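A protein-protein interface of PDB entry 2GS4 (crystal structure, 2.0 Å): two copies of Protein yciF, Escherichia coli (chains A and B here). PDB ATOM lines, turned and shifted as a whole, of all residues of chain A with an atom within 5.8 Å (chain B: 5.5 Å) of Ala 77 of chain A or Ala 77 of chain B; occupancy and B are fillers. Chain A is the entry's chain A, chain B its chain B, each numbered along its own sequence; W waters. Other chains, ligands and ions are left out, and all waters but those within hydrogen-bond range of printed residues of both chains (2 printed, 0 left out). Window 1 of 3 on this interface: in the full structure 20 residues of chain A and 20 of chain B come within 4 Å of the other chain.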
ATOM      1  N   CYS A  75      12.000  -4.310  -9.145  1.00  0.00           N
ATOM      2  CA  CYS A  75      11.925  -3.906  -7.745  1.00  0.00           C
ATOM      3  C   CYS A  75      13.270  -4.234  -7.099  1.00  0.00           C
ATOM      4  O   CYS A  75      13.579  -5.400  -6.823  1.00  0.00           O
ATOM      5  CB  CYS A  75      10.785  -4.654  -7.040  1.00  0.00           C
ATOM      6  SG  CYS A  75      10.637  -4.336  -5.264  1.00  0.00           S
ATOM      7  N   VAL A  76      14.057  -3.189  -6.861  1.00  0.00           N
ATOM      8  CA  VAL A  76      15.384  -3.315  -6.272  1.00  0.00           C
ATOM      9  C   VAL A  76      15.346  -3.832  -4.834  1.00  0.00           C
ATOM     10  O   VAL A  76      16.248  -4.551  -4.403  1.00  0.00           O
ATOM     11  CB  VAL A  76      16.114  -1.953  -6.363  1.00  0.00           C
ATOM     12  CG1 VAL A  76      17.390  -1.960  -5.554  1.00  0.00           C
ATOM     13  CG2 VAL A  76      16.429  -1.666  -7.833  1.00  0.00           C
ATOM     14  N   ALA A  77      14.305  -3.467  -4.093  1.00  0.00           N
ATOM     15  CA  ALA A  77      14.167  -3.918  -2.716  1.00  0.00           C
ATOM     16  C   ALA A  77      14.056  -5.446  -2.678  1.00  0.00           C
ATOM     17  O   ALA A  77      14.792  -6.101  -1.952  1.00  0.00           O
ATOM     18  CB  ALA A  77      12.941  -3.281  -2.076  1.00  0.00           C
ATOM     19  N   MET A  78      13.141  -6.018  -3.457  1.00  0.00           N
ATOM     20  CA  MET A  78      13.000  -7.475  -3.446  1.00  0.00           C
ATOM     21  C   MET A  78      14.262  -8.173  -3.921  1.00  0.00           C
ATOM     22  O   MET A  78      14.625  -9.230  -3.407  1.00  0.00           O
ATOM     23  CB  MET A  78      11.830  -7.933  -4.320  1.00  0.00           C
ATOM     24  CG  MET A  78      11.670  -9.453  -4.309  1.00  0.00           C
ATOM     25  SD  MET A  78      11.367 -10.155  -2.534  1.00  0.00           S
ATOM     26  CE  MET A  78       9.488  -9.716  -2.395  1.00  0.00           C
ATOM     27  N   GLU A  79      14.920  -7.584  -4.915  1.00  0.00           N
ATOM     28  CA  GLU A  79      16.149  -8.131  -5.475  1.00  0.00           C
ATOM     29  C   GLU A  79      17.174  -8.288  -4.344  1.00  0.00           C
ATOM     30  O   GLU A  79      17.834  -9.326  -4.230  1.00  0.00           O
ATOM     31  CB  GLU A  79      16.658  -7.182  -6.573  1.00  0.00           C
ATOM     32  CG  GLU A  79      17.924  -7.566  -7.302  1.00  0.00           C
ATOM     33  CD  GLU A  79      18.316  -6.504  -8.329  1.00  0.00           C
ATOM     34  OE1 GLU A  79      18.195  -6.763  -9.545  1.00  0.00           O
ATOM     35  OE2 GLU A  79      18.733  -5.400  -7.914  1.00  0.00           O
ATOM     36  N   GLY A  80      17.285  -7.269  -3.496  1.00  0.00           N
ATOM     37  CA  GLY A  80      18.222  -7.339  -2.389  1.00  0.00           C
ATOM     38  C   GLY A  80      17.832  -8.402  -1.371  1.00  0.00           C
ATOM     39  O   GLY A  80      18.689  -9.129  -0.868  1.00  0.00           O
ATOM     40  N   LEU A  81      16.538  -8.503  -1.072  1.00  0.00           N
ATOM     41  CA  LEU A  81      16.054  -9.480  -0.102  1.00  0.00           C
ATOM     42  C   LEU A  81      16.279 -10.904  -0.607  1.00  0.00           C
ATOM     43  O   LEU A  81      16.534 -11.826   0.179  1.00  0.00           O
ATOM     44  CB  LEU A  81      14.566  -9.234   0.188  1.00  0.00           C
ATOM     45  CG  LEU A  81      14.291  -7.897   0.891  1.00  0.00           C
ATOM     46  CD1 LEU A  81      12.789  -7.645   1.036  1.00  0.00           C
ATOM     47  CD2 LEU A  81      14.960  -7.913   2.251  1.00  0.00           C
ATOM     48  N   ILE A  82      16.197 -11.071  -1.924  1.00  0.00           N
ATOM     49  CA  ILE A  82      16.402 -12.369  -2.532  1.00  0.00           C
ATOM     50  C   ILE A  82      17.904 -12.688  -2.534  1.00  0.00           C
ATOM     51  O   ILE A  82      18.300 -13.831  -2.318  1.00  0.00           O
ATOM     52  CB  ILE A  82      15.751 -12.388  -3.939  1.00  0.00           C
ATOM     53  CG1 ILE A  82      14.233 -12.540  -3.757  1.00  0.00           C
ATOM     54  CG2 ILE A  82      16.342 -13.490  -4.806  1.00  0.00           C
ATOM     55  CD1 ILE A  82      13.389 -12.385  -5.005  1.00  0.00           C
ATOM     56  N   TYR A 112       8.633  -7.372   4.356  1.00  0.00           N
ATOM     57  CA  TYR A 112       8.509  -6.482   3.211  1.00  0.00           C
ATOM     58  C   TYR A 112       7.164  -6.633   2.495  1.00  0.00           C
ATOM     59  O   TYR A 112       6.496  -5.650   2.206  1.00  0.00           O
ATOM     60  CB  TYR A 112       9.636  -6.754   2.215  1.00  0.00           C
ATOM     61  CG  TYR A 112       9.609  -5.879   0.978  1.00  0.00           C
ATOM     62  CD1 TYR A 112      10.127  -4.585   1.001  1.00  0.00           C
ATOM     63  CD2 TYR A 112       9.085  -6.356  -0.223  1.00  0.00           C
ATOM     64  CE1 TYR A 112      10.129  -3.790  -0.144  1.00  0.00           C
ATOM     65  CE2 TYR A 112       9.081  -5.573  -1.371  1.00  0.00           C
ATOM     66  CZ  TYR A 112       9.607  -4.292  -1.325  1.00  0.00           C
ATOM     67  OH  TYR A 112       9.636  -3.521  -2.464  1.00  0.00           O
ATOM     68  N   CYS B  75      13.526  -1.127   8.608  1.00  0.00           N
ATOM     69  CA  CYS B  75      13.329  -1.145   7.172  1.00  0.00           C
ATOM     70  C   CYS B  75      14.179  -2.296   6.697  1.00  0.00           C
ATOM     71  O   CYS B  75      15.406  -2.214   6.645  1.00  0.00           O
ATOM     72  CB  CYS B  75      13.803   0.156   6.533  1.00  0.00           C
ATOM     73  SG  CYS B  75      13.921   0.083   4.719  1.00  0.00           S
ATOM     74  N   VAL B  76      13.490  -3.381   6.378  1.00  0.00           N
ATOM     75  CA  VAL B  76      14.103  -4.612   5.929  1.00  0.00           C
ATOM     76  C   VAL B  76      14.756  -4.513   4.543  1.00  0.00           C
ATOM     77  O   VAL B  76      15.796  -5.135   4.304  1.00  0.00           O
ATOM     78  CB  VAL B  76      13.034  -5.732   6.019  1.00  0.00           C
ATOM     79  CG1 VAL B  76      13.441  -6.960   5.259  1.00  0.00           C
ATOM     80  CG2 VAL B  76      12.808  -6.072   7.507  1.00  0.00           C
ATOM     81  N   ALA B  77      14.172  -3.724   3.645  1.00  0.00           N
ATOM     82  CA  ALA B  77      14.736  -3.565   2.302  1.00  0.00           C
ATOM     83  C   ALA B  77      16.167  -3.011   2.350  1.00  0.00           C
ATOM     84  O   ALA B  77      17.045  -3.480   1.632  1.00  0.00           O
ATOM     85  CB  ALA B  77      13.856  -2.651   1.461  1.00  0.00           C
ATOM     86  N   MET B  78      16.401  -2.017   3.204  1.00  0.00           N
ATOM     87  CA  MET B  78      17.727  -1.426   3.320  1.00  0.00           C
ATOM     88  C   MET B  78      18.744  -2.439   3.851  1.00  0.00           C
ATOM     89  O   MET B  78      19.915  -2.390   3.469  1.00  0.00           O
ATOM     90  CB  MET B  78      17.674  -0.167   4.207  1.00  0.00           C
ATOM     91  CG  MET B  78      19.001   0.627   4.301  1.00  0.00           C
ATOM     92  SD  MET B  78      19.852   1.131   2.617  1.00  0.00           S
ATOM     93  CE  MET B  78      19.135   2.918   2.398  1.00  0.00           C
ATOM     94  N   GLU B  79      18.315  -3.349   4.729  1.00  0.00           N
ATOM     95  CA  GLU B  79      19.229  -4.366   5.244  1.00  0.00           C
ATOM     96  C   GLU B  79      19.798  -5.137   4.052  1.00  0.00           C
ATOM     97  O   GLU B  79      21.005  -5.348   3.946  1.00  0.00           O
ATOM     98  CB  GLU B  79      18.496  -5.354   6.165  1.00  0.00           C
ATOM     99  CG  GLU B  79      18.103  -4.819   7.546  1.00  0.00           C
ATOM    100  CD  GLU B  79      17.211  -5.787   8.300  1.00  0.00           C
ATOM    101  OE1 GLU B  79      16.817  -5.471   9.432  1.00  0.00           O
ATOM    102  OE2 GLU B  79      16.895  -6.869   7.767  1.00  0.00           O
ATOM    103  N   GLY B  80      18.906  -5.556   3.162  1.00  0.00           N
ATOM    104  CA  GLY B  80      19.313  -6.307   1.987  1.00  0.00           C
ATOM    105  C   GLY B  80      20.252  -5.554   1.058  1.00  0.00           C
ATOM    106  O   GLY B  80      21.232  -6.126   0.563  1.00  0.00           O
ATOM    107  N   LEU B  81      19.966  -4.275   0.810  1.00  0.00           N
ATOM    108  CA  LEU B  81      20.809  -3.477  -0.069  1.00  0.00           C
ATOM    109  C   LEU B  81      22.184  -3.253   0.563  1.00  0.00           C
ATOM    110  O   LEU B  81      23.202  -3.256  -0.138  1.00  0.00           O
ATOM    111  CB  LEU B  81      20.128  -2.137  -0.384  1.00  0.00           C
ATOM    112  CG  LEU B  81      18.798  -2.228  -1.143  1.00  0.00           C
ATOM    113  CD1 LEU B  81      18.279  -0.820  -1.432  1.00  0.00           C
ATOM    114  CD2 LEU B  81      18.994  -2.991  -2.448  1.00  0.00           C
ATOM    115  N   ILE B  82      22.216  -3.061   1.884  1.00  0.00           N
ATOM    116  CA  ILE B  82      23.484  -2.866   2.569  1.00  0.00           C
ATOM    117  C   ILE B  82      24.284  -4.182   2.488  1.00  0.00           C
ATOM    118  O   ILE B  82      25.513  -4.165   2.388  1.00  0.00           O
ATOM    119  CB  ILE B  82      23.260  -2.421   4.056  1.00  0.00           C
ATOM    120  CG1 ILE B  82      22.967  -0.908   4.101  1.00  0.00           C
ATOM    121  CG2 ILE B  82      24.488  -2.766   4.908  1.00  0.00           C
ATOM    122  CD1 ILE B  82      22.531  -0.350   5.471  1.00  0.00           C
ATOM    123  N   TYR B 112      16.708   2.998  -4.633  1.00  0.00           N
ATOM    124  CA  TYR B 112      15.707   2.807  -3.594  1.00  0.00           C
ATOM    125  C   TYR B 112      15.353   4.097  -2.845  1.00  0.00           C
ATOM    126  O   TYR B 112      14.174   4.414  -2.672  1.00  0.00           O
ATOM    127  CB  TYR B 112      16.213   1.764  -2.613  1.00  0.00           C
ATOM    128  CG  TYR B 112      15.295   1.508  -1.454  1.00  0.00           C
ATOM    129  CD1 TYR B 112      14.132   0.753  -1.607  1.00  0.00           C
ATOM    130  CD2 TYR B 112      15.599   2.007  -0.192  1.00  0.00           C
ATOM    131  CE1 TYR B 112      13.298   0.498  -0.520  1.00  0.00           C
ATOM    132  CE2 TYR B 112      14.772   1.762   0.898  1.00  0.00           C
ATOM    133  CZ  TYR B 112      13.629   1.006   0.727  1.00  0.00           C
ATOM    134  OH  TYR B 112      12.841   0.746   1.816  1.00  0.00           O
HETATM  135  O   HOH W   1      21.290  -8.684  -0.198  1.00  0.00           O
HETATM  136  O   HOH W   2      16.838  -5.343  -0.165  1.00  0.00           O
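Val 76 of chain A touches Leu 81 of chain B, and with the chains exchanged Leu 81 of chain A touches Val 76 of chain B.
Ala 77 of chain A touches its own counterpart, Ala 77 of chain B.
CG1 of Val 76 of chain A touches CD2 of Leu 81 of chain B (3.6 Å).
CB of Ala 77 of chain B touches CB of Ala 77 of chain A, 3.7 Å away.
Val 76 of chain B touches Leu 81 of chain A.
Water W2 lies within hydrogen-bond range of the backbone carbonyl oxygen (O) of Ala 77 of chain B (2.6 Å), the backbone carbonyl oxygen (O) of Ala 77 of chain A (2.8 Å), the backbone NH (N) of Leu 81 of chain A (3.3 Å) and the backbone NH (N) of Leu 81 of chain B (3.4 Å).
Water W1 lies within hydrogen-bond range of the backbone carbonyl oxygen of Gly 80 of chain B (2.7 Å) and the backbone carbonyl oxygen of Gly 80 of chain A (2.7 Å).
Of the 9 printed residues of chain A, 3 touch a printed residue of chain B.
Among the printed residues, no Asp or Glu carboxylate lies within 4 Å of a Lys or Arg side-chain nitrogen of the other chain.
Of chain B, only Ala 77 (3.7 Å) comes within 4 Å of Ala 77 of chain A.
Printed residues of chain A within 4 Å of Ala 77 of chain B: Ala 77.
Printed residues of chain A within 4 Å of Val 76 of chain B: Leu 81 (3.5 Å).
Of the printed residues of chain B, Val 76 of chain A touches Leu 81 (3.6 Å).
Printed residues of chain A within 4 Å of Leu 81 of chain B: Val 76.
Printed residues of chain B within 4 Å of Leu 81 of chain A: Val 76.
The nearest residue of chain B that does not touch Ala 77 of chain A is Tyr 112 of chain B (4.1 Å).
The nearest printed residue of chain B that does not touch Val 76 of chain A is Tyr 112 of chain B (4.9 Å).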
